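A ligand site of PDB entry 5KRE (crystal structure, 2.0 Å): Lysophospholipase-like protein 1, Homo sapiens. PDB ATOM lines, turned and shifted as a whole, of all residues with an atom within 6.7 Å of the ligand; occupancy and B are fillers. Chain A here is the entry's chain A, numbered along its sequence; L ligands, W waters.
The backbone NH (N) of Met 127 is in hydrogen-bond range of an oxygen (O1) of the ligand (2.8 Å).
The backbone NH (N) of Ser 32 sits at hydrogen-bond distance from an oxygen (O1) of the ligand, at 2.9 Å.
O1 of the ligand sits at hydrogen-bond distance from OG of Ser 32 (3.4 Å).
The side-chain hydroxyl (OG) of Ser 126 is covalently linked to a carbon (C12) of the ligand.
The backbone NH (N) of Gly 31 lies close to the backbone carbonyl oxygen (O) of Phe 125, at 3.5 Å.
N of Ser 126 lies close to O of Ser 150 (3.5 Å).
The side-chain carboxylate (OD1) of Asp 181 lies within hydrogen-bond range of the backbone NH (N) of Val 184.
OG of Ser 151 sits at hydrogen-bond distance from O of Ser 126 (2.7 Å).
OG of Ser 126 lies within hydrogen-bond range of NE2 of His 213 (3.3 Å).
OD1 of Asp 181 lies within hydrogen-bond range of N of Leu 183.
Gly 31 touches the ligand (CA to O1, 3.7 Å).
OH of Tyr 68 touches C10 of the ligand, at 3.6 Å.
NE of Arg 82 touches C10 of the ligand, 3.2 Å away.
CG2 of Ile 85 touches C9 of the ligand, 3.7 Å away.
CE1 of Phe 152 touches C5 of the ligand, 3.8 Å away.
Leu 183 touches the ligand.
CG2 of Val 184 touches C5 of the ligand (3.4 Å).
Hydrophobic or aromatic side chains that line the ligand: Ile 85, Met 127, Phe 152, Leu 183 and Val 184.
Within 4 Å of the ligand: Gly 31, Ser 32, Tyr 68, Arg 82, Ile 85, Ser 126, Met 127, Phe 152, Leu 183 and Val 184.
The nearest printed residue that does not touch the ligand is His 213 (4.02 Å).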
ATOM      1  N   HIS A  30      12.500  -3.667  13.248  1.00  0.00           N
ATOM      2  CA  HIS A  30      13.546  -4.003  14.230  1.00  0.00           C
ATOM      3  C   HIS A  30      14.823  -3.168  14.027  1.00  0.00           C
ATOM      4  O   HIS A  30      15.021  -2.567  12.957  1.00  0.00           O
ATOM      5  CB  HIS A  30      13.839  -5.530  14.142  1.00  0.00           C
ATOM      6  CG  HIS A  30      14.498  -5.971  12.878  1.00  0.00           C
ATOM      7  ND1 HIS A  30      15.860  -5.792  12.678  1.00  0.00           N
ATOM      8  CD2 HIS A  30      13.979  -6.598  11.788  1.00  0.00           C
ATOM      9  CE1 HIS A  30      16.131  -6.311  11.483  1.00  0.00           C
ATOM     10  NE2 HIS A  30      15.031  -6.806  10.909  1.00  0.00           N
ATOM     11  N   GLY A  31      15.685  -3.149  15.048  1.00  0.00           N
ATOM     12  CA  GLY A  31      16.968  -2.462  15.009  1.00  0.00           C
ATOM     13  C   GLY A  31      18.039  -3.319  14.366  1.00  0.00           C
ATOM     14  O   GLY A  31      17.770  -4.468  13.977  1.00  0.00           O
ATOM     15  N   SER A  32      19.268  -2.795  14.223  1.00  0.00           N
ATOM     16  CA  SER A  32      20.360  -3.538  13.601  1.00  0.00           C
ATOM     17  C   SER A  32      20.596  -4.932  14.215  1.00  0.00           C
ATOM     18  O   SER A  32      20.529  -5.107  15.442  1.00  0.00           O
ATOM     19  CB  SER A  32      21.660  -2.734  13.647  1.00  0.00           C
ATOM     20  OG  SER A  32      22.009  -2.459  14.992  1.00  0.00           O
ATOM     21  N   GLY A  33      20.854  -5.914  13.344  1.00  0.00           N
ATOM     22  CA  GLY A  33      21.182  -7.287  13.726  1.00  0.00           C
ATOM     23  C   GLY A  33      20.068  -8.160  14.302  1.00  0.00           C
ATOM     24  O   GLY A  33      20.332  -9.294  14.682  1.00  0.00           O
ATOM     25  N   TYR A  68      27.305  -4.759   6.075  1.00  0.00           N
ATOM     26  CA  TYR A  68      27.144  -3.617   6.958  1.00  0.00           C
ATOM     27  C   TYR A  68      28.546  -3.064   7.217  1.00  0.00           C
ATOM     28  O   TYR A  68      29.395  -3.768   7.779  1.00  0.00           O
ATOM     29  CB  TYR A  68      26.405  -4.045   8.245  1.00  0.00           C
ATOM     30  CG  TYR A  68      26.026  -2.911   9.168  1.00  0.00           C
ATOM     31  CD1 TYR A  68      25.347  -1.792   8.690  1.00  0.00           C
ATOM     32  CD2 TYR A  68      26.273  -2.995  10.535  1.00  0.00           C
ATOM     33  CE1 TYR A  68      25.025  -0.737   9.539  1.00  0.00           C
ATOM     34  CE2 TYR A  68      25.930  -1.953  11.400  1.00  0.00           C
ATOM     35  CZ  TYR A  68      25.307  -0.820  10.892  1.00  0.00           C
ATOM     36  OH  TYR A  68      24.981   0.228  11.717  1.00  0.00           O
ATOM     37  N   VAL A  78      20.241  -5.709   8.607  1.00  0.00           N
ATOM     38  CA  VAL A  78      20.188  -4.242   8.712  1.00  0.00           C
ATOM     39  C   VAL A  78      19.313  -3.724   7.586  1.00  0.00           C
ATOM     40  O   VAL A  78      19.411  -4.242   6.455  1.00  0.00           O
ATOM     41  CB  VAL A  78      21.602  -3.585   8.728  1.00  0.00           C
ATOM     42  CG1 VAL A  78      22.362  -3.939  10.009  1.00  0.00           C
ATOM     43  CG2 VAL A  78      22.434  -3.935   7.486  1.00  0.00           C
ATOM     44  N   PHE A  80      19.489  -0.800   6.151  1.00  0.00           N
ATOM     45  CA  PHE A  80      20.333   0.004   5.265  1.00  0.00           C
ATOM     46  C   PHE A  80      21.735   0.069   5.819  1.00  0.00           C
ATOM     47  O   PHE A  80      21.990  -0.390   6.932  1.00  0.00           O
ATOM     48  CB  PHE A  80      19.726   1.430   5.081  1.00  0.00           C
ATOM     49  CG  PHE A  80      19.513   2.199   6.373  1.00  0.00           C
ATOM     50  CD1 PHE A  80      20.535   2.945   6.943  1.00  0.00           C
ATOM     51  CD2 PHE A  80      18.272   2.188   7.012  1.00  0.00           C
ATOM     52  CE1 PHE A  80      20.353   3.608   8.161  1.00  0.00           C
ATOM     53  CE2 PHE A  80      18.077   2.885   8.208  1.00  0.00           C
ATOM     54  CZ  PHE A  80      19.119   3.592   8.779  1.00  0.00           C
ATOM     55  N   ARG A  82      25.411   2.229   6.847  1.00  0.00           N
ATOM     56  CA  ARG A  82      25.916   3.470   7.439  1.00  0.00           C
ATOM     57  C   ARG A  82      27.419   3.479   7.256  1.00  0.00           C
ATOM     58  O   ARG A  82      28.055   2.432   7.396  1.00  0.00           O
ATOM     59  CB  ARG A  82      25.611   3.551   8.940  1.00  0.00           C
ATOM     60  CG  ARG A  82      24.143   3.831   9.234  1.00  0.00           C
ATOM     61  CD  ARG A  82      23.985   4.180  10.700  1.00  0.00           C
ATOM     62  NE  ARG A  82      22.596   4.492  11.028  1.00  0.00           N
ATOM     63  CZ  ARG A  82      22.058   5.692  10.906  1.00  0.00           C
ATOM     64  NH1 ARG A  82      22.790   6.711  10.470  1.00  0.00           N
ATOM     65  NH2 ARG A  82      20.786   5.887  11.207  1.00  0.00           N
ATOM     66  N   LYS A  84      29.585   5.295   9.187  1.00  0.00           N
ATOM     67  CA  LYS A  84      30.115   5.452  10.547  1.00  0.00           C
ATOM     68  C   LYS A  84      28.951   5.675  11.489  1.00  0.00           C
ATOM     69  O   LYS A  84      27.899   6.160  11.062  1.00  0.00           O
ATOM     70  CB  LYS A  84      30.970   6.747  10.623  1.00  0.00           C
ATOM     71  CG  LYS A  84      32.266   6.760   9.837  1.00  0.00           C
ATOM     72  CD  LYS A  84      32.779   8.177   9.727  1.00  0.00           C
ATOM     73  CE  LYS A  84      33.603   8.384   8.476  1.00  0.00           C
ATOM     74  NZ  LYS A  84      34.897   7.647   8.515  1.00  0.00           N
ATOM     75  N   ILE A  85      29.147   5.414  12.795  1.00  0.00           N
ATOM     76  CA  ILE A  85      28.087   5.653  13.768  1.00  0.00           C
ATOM     77  C   ILE A  85      28.214   7.091  14.302  1.00  0.00           C
ATOM     78  O   ILE A  85      28.907   7.334  15.290  1.00  0.00           O
ATOM     79  CB  ILE A  85      27.981   4.564  14.877  1.00  0.00           C
ATOM     80  CG1 ILE A  85      27.945   3.091  14.303  1.00  0.00           C
ATOM     81  CG2 ILE A  85      26.778   4.830  15.808  1.00  0.00           C
ATOM     82  CD1 ILE A  85      26.925   2.813  13.132  1.00  0.00           C
ATOM     83  N   THR A  86      27.558   8.019  13.596  1.00  0.00           N
ATOM     84  CA  THR A  86      27.489   9.455  13.891  1.00  0.00           C
ATOM     85  C   THR A  86      26.406  10.062  13.032  1.00  0.00           C
ATOM     86  O   THR A  86      26.040   9.483  12.007  1.00  0.00           O
ATOM     87  CB  THR A  86      28.855  10.202  13.664  1.00  0.00           C
ATOM     88  OG1 THR A  86      28.651  11.584  13.962  1.00  0.00           O
ATOM     89  CG2 THR A  86      29.364  10.080  12.233  1.00  0.00           C
ATOM     90  N   PHE A 125      12.662   0.616  15.909  1.00  0.00           N
ATOM     91  CA  PHE A 125      13.665   0.799  16.930  1.00  0.00           C
ATOM     92  C   PHE A 125      14.999   0.993  16.253  1.00  0.00           C
ATOM     93  O   PHE A 125      15.312   0.273  15.298  1.00  0.00           O
ATOM     94  CB  PHE A 125      13.700  -0.427  17.885  1.00  0.00           C
ATOM     95  CG  PHE A 125      14.846  -0.420  18.872  1.00  0.00           C
ATOM     96  CD1 PHE A 125      14.798   0.371  20.020  1.00  0.00           C
ATOM     97  CD2 PHE A 125      15.988  -1.185  18.643  1.00  0.00           C
ATOM     98  CE1 PHE A 125      15.867   0.384  20.926  1.00  0.00           C
ATOM     99  CE2 PHE A 125      17.066  -1.170  19.551  1.00  0.00           C
ATOM    100  CZ  PHE A 125      16.993  -0.385  20.679  1.00  0.00           C
ATOM    101  N   SER A 126      15.789   1.992  16.720  1.00  0.00           N
ATOM    102  CA  SER A 126      17.118   2.282  16.195  1.00  0.00           C
ATOM    103  C   SER A 126      17.010   2.483  14.657  1.00  0.00           C
ATOM    104  O   SER A 126      16.279   3.364  14.229  1.00  0.00           O
ATOM    105  CB  SER A 126      18.096   1.191  16.624  1.00  0.00           C
ATOM    106  OG  SER A 126      19.468   1.531  16.453  1.00  0.00           O
ATOM    107  N   MET A 127      17.648   1.640  13.828  1.00  0.00           N
ATOM    108  CA  MET A 127      17.583   1.667  12.365  1.00  0.00           C
ATOM    109  C   MET A 127      16.146   1.631  11.799  1.00  0.00           C
ATOM    110  O   MET A 127      15.848   2.274  10.785  1.00  0.00           O
ATOM    111  CB  MET A 127      18.316   0.437  11.866  1.00  0.00           C
ATOM    112  CG  MET A 127      19.089   0.681  10.703  1.00  0.00           C
ATOM    113  SD  MET A 127      20.138  -0.743  10.387  1.00  0.00           S
ATOM    114  CE  MET A 127      21.581   0.106  10.047  1.00  0.00           C
ATOM    115  N   GLY A 128      15.276   0.885  12.466  1.00  0.00           N
ATOM    116  CA  GLY A 128      13.868   0.784  12.112  1.00  0.00           C
ATOM    117  C   GLY A 128      13.119   2.110  12.179  1.00  0.00           C
ATOM    118  O   GLY A 128      12.234   2.363  11.356  1.00  0.00           O
ATOM    119  N   SER A 150      14.702   5.318  19.987  1.00  0.00           N
ATOM    120  CA  SER A 150      16.176   5.350  20.038  1.00  0.00           C
ATOM    121  C   SER A 150      16.748   5.430  18.637  1.00  0.00           C
ATOM    122  O   SER A 150      17.559   4.570  18.250  1.00  0.00           O
ATOM    123  CB  SER A 150      16.720   4.112  20.760  1.00  0.00           C
ATOM    124  OG  SER A 150      16.112   3.990  22.042  1.00  0.00           O
ATOM    125  N   SER A 151      16.309   6.447  17.861  1.00  0.00           N
ATOM    126  CA  SER A 151      16.703   6.624  16.451  1.00  0.00           C
ATOM    127  C   SER A 151      17.189   8.046  16.183  1.00  0.00           C
ATOM    128  O   SER A 151      17.007   8.923  17.012  1.00  0.00           O
ATOM    129  CB  SER A 151      15.483   6.386  15.553  1.00  0.00           C
ATOM    130  OG  SER A 151      14.926   5.096  15.730  1.00  0.00           O
ATOM    131  N   PHE A 152      17.712   8.283  14.972  1.00  0.00           N
ATOM    132  CA  PHE A 152      18.190   9.606  14.564  1.00  0.00           C
ATOM    133  C   PHE A 152      18.321   9.659  13.051  1.00  0.00           C
ATOM    134  O   PHE A 152      18.424   8.627  12.396  1.00  0.00           O
ATOM    135  CB  PHE A 152      19.580   9.912  15.207  1.00  0.00           C
ATOM    136  CG  PHE A 152      20.759   9.129  14.658  1.00  0.00           C
ATOM    137  CD1 PHE A 152      20.982   7.804  15.036  1.00  0.00           C
ATOM    138  CD2 PHE A 152      21.661   9.722  13.775  1.00  0.00           C
ATOM    139  CE1 PHE A 152      22.083   7.102  14.564  1.00  0.00           C
ATOM    140  CE2 PHE A 152      22.752   8.996  13.277  1.00  0.00           C
ATOM    141  CZ  PHE A 152      22.969   7.705  13.693  1.00  0.00           C
ATOM    142  N   ASP A 181      21.751   6.702  26.606  1.00  0.00           N
ATOM    143  CA  ASP A 181      22.118   5.870  25.436  1.00  0.00           C
ATOM    144  C   ASP A 181      23.507   6.255  24.880  1.00  0.00           C
ATOM    145  O   ASP A 181      23.720   7.399  24.473  1.00  0.00           O
ATOM    146  CB  ASP A 181      21.028   5.980  24.368  1.00  0.00           C
ATOM    147  CG  ASP A 181      21.129   5.051  23.170  1.00  0.00           C
ATOM    148  OD1 ASP A 181      22.244   4.535  22.905  1.00  0.00           O
ATOM    149  OD2 ASP A 181      20.121   4.864  22.488  1.00  0.00           O
ATOM    150  N   GLU A 182      24.447   5.284  24.860  1.00  0.00           N
ATOM    151  CA  GLU A 182      25.815   5.502  24.374  1.00  0.00           C
ATOM    152  C   GLU A 182      26.009   5.038  22.914  1.00  0.00           C
ATOM    153  O   GLU A 182      27.091   5.242  22.358  1.00  0.00           O
ATOM    154  CB  GLU A 182      26.830   4.804  25.299  1.00  0.00           C
ATOM    155  CG  GLU A 182      26.929   5.448  26.685  1.00  0.00           C
ATOM    156  CD  GLU A 182      27.587   6.822  26.718  1.00  0.00           C
ATOM    157  OE1 GLU A 182      28.421   7.115  25.833  1.00  0.00           O
ATOM    158  OE2 GLU A 182      27.258   7.604  27.638  1.00  0.00           O
ATOM    159  N   LEU A 183      24.972   4.435  22.309  1.00  0.00           N
ATOM    160  CA  LEU A 183      24.990   3.943  20.909  1.00  0.00           C
ATOM    161  C   LEU A 183      24.428   5.008  19.981  1.00  0.00           C
ATOM    162  O   LEU A 183      25.090   5.373  18.999  1.00  0.00           O
ATOM    163  CB  LEU A 183      24.226   2.606  20.755  1.00  0.00           C
ATOM    164  CG  LEU A 183      24.626   1.438  21.662  1.00  0.00           C
ATOM    165  CD1 LEU A 183      24.210   0.130  21.069  1.00  0.00           C
ATOM    166  CD2 LEU A 183      26.098   1.396  21.975  1.00  0.00           C
ATOM    167  N   VAL A 184      23.216   5.500  20.281  1.00  0.00           N
ATOM    168  CA  VAL A 184      22.575   6.648  19.611  1.00  0.00           C
ATOM    169  C   VAL A 184      22.569   7.742  20.691  1.00  0.00           C
ATOM    170  O   VAL A 184      21.814   7.653  21.667  1.00  0.00           O
ATOM    171  CB  VAL A 184      21.139   6.394  19.071  1.00  0.00           C
ATOM    172  CG1 VAL A 184      20.593   7.644  18.393  1.00  0.00           C
ATOM    173  CG2 VAL A 184      21.109   5.209  18.100  1.00  0.00           C
ATOM    174  N   TRP A 188      21.738  13.445  19.239  1.00  0.00           N
ATOM    175  CA  TRP A 188      21.401  13.139  17.829  1.00  0.00           C
ATOM    176  C   TRP A 188      19.909  12.999  17.642  1.00  0.00           C
ATOM    177  O   TRP A 188      19.368  13.482  16.650  1.00  0.00           O
ATOM    178  CB  TRP A 188      22.098  11.864  17.297  1.00  0.00           C
ATOM    179  CG  TRP A 188      23.587  11.808  17.461  1.00  0.00           C
ATOM    180  CD1 TRP A 188      24.453  12.839  17.707  1.00  0.00           C
ATOM    181  CD2 TRP A 188      24.403  10.638  17.311  1.00  0.00           C
ATOM    182  NE1 TRP A 188      25.743  12.376  17.767  1.00  0.00           N
ATOM    183  CE2 TRP A 188      25.743  11.017  17.557  1.00  0.00           C
ATOM    184  CE3 TRP A 188      24.119   9.277  17.105  1.00  0.00           C
ATOM    185  CZ2 TRP A 188      26.797  10.102  17.537  1.00  0.00           C
ATOM    186  CZ3 TRP A 188      25.154   8.364  17.118  1.00  0.00           C
ATOM    187  CH2 TRP A 188      26.484   8.778  17.328  1.00  0.00           C
ATOM    188  N   HIS A 213      20.241   2.119  25.415  1.00  0.00           N
ATOM    189  CA  HIS A 213      19.800   1.750  24.058  1.00  0.00           C
ATOM    190  C   HIS A 213      19.017   0.487  24.224  1.00  0.00           C
ATOM    191  O   HIS A 213      19.533  -0.624  24.087  1.00  0.00           O
ATOM    192  CB  HIS A 213      20.990   1.511  23.112  1.00  0.00           C
ATOM    193  CG  HIS A 213      20.600   1.441  21.652  1.00  0.00           C
ATOM    194  ND1 HIS A 213      20.234   2.575  20.945  1.00  0.00           N
ATOM    195  CD2 HIS A 213      20.606   0.384  20.807  1.00  0.00           C
ATOM    196  CE1 HIS A 213      19.994   2.170  19.707  1.00  0.00           C
ATOM    197  NE2 HIS A 213      20.217   0.860  19.578  1.00  0.00           N
HETATM  198  C1  LIG L   1      23.528   1.447  16.805  1.00  0.00           C
HETATM  199  C2  LIG L   1      22.268   2.119  16.275  1.00  0.00           C
HETATM  200  C3  LIG L   1      25.785   1.572  17.649  1.00  0.00           C
HETATM  201  C4  LIG L   1      23.183   3.215  14.173  1.00  0.00           C
HETATM  202  C5  LIG L   1      22.460   3.422  15.492  1.00  0.00           C
HETATM  203  C6  LIG L   1      25.849   0.204  17.757  1.00  0.00           C
HETATM  204  C7  LIG L   1      24.747  -0.560  17.408  1.00  0.00           C
HETATM  205  C8  LIG L   1      23.590   0.062  16.940  1.00  0.00           C
HETATM  206  C9  LIG L   1      24.637   2.196  17.183  1.00  0.00           C
HETATM  207  C10 LIG L   1      22.471   2.195  13.307  1.00  0.00           C
HETATM  208  C11 LIG L   1      22.212   0.928  14.072  1.00  0.00           C
HETATM  209  N1  LIG L   1      21.548   1.236  15.354  1.00  0.00           N
HETATM  210  C12 LIG L   1      20.294   0.799  15.564  1.00  0.00           C
HETATM  211  O1  LIG L   1      19.703   0.028  14.838  1.00  0.00           O
HETATM  212  O   HOH W   1      25.736  -0.286  14.211  1.00  0.00           O
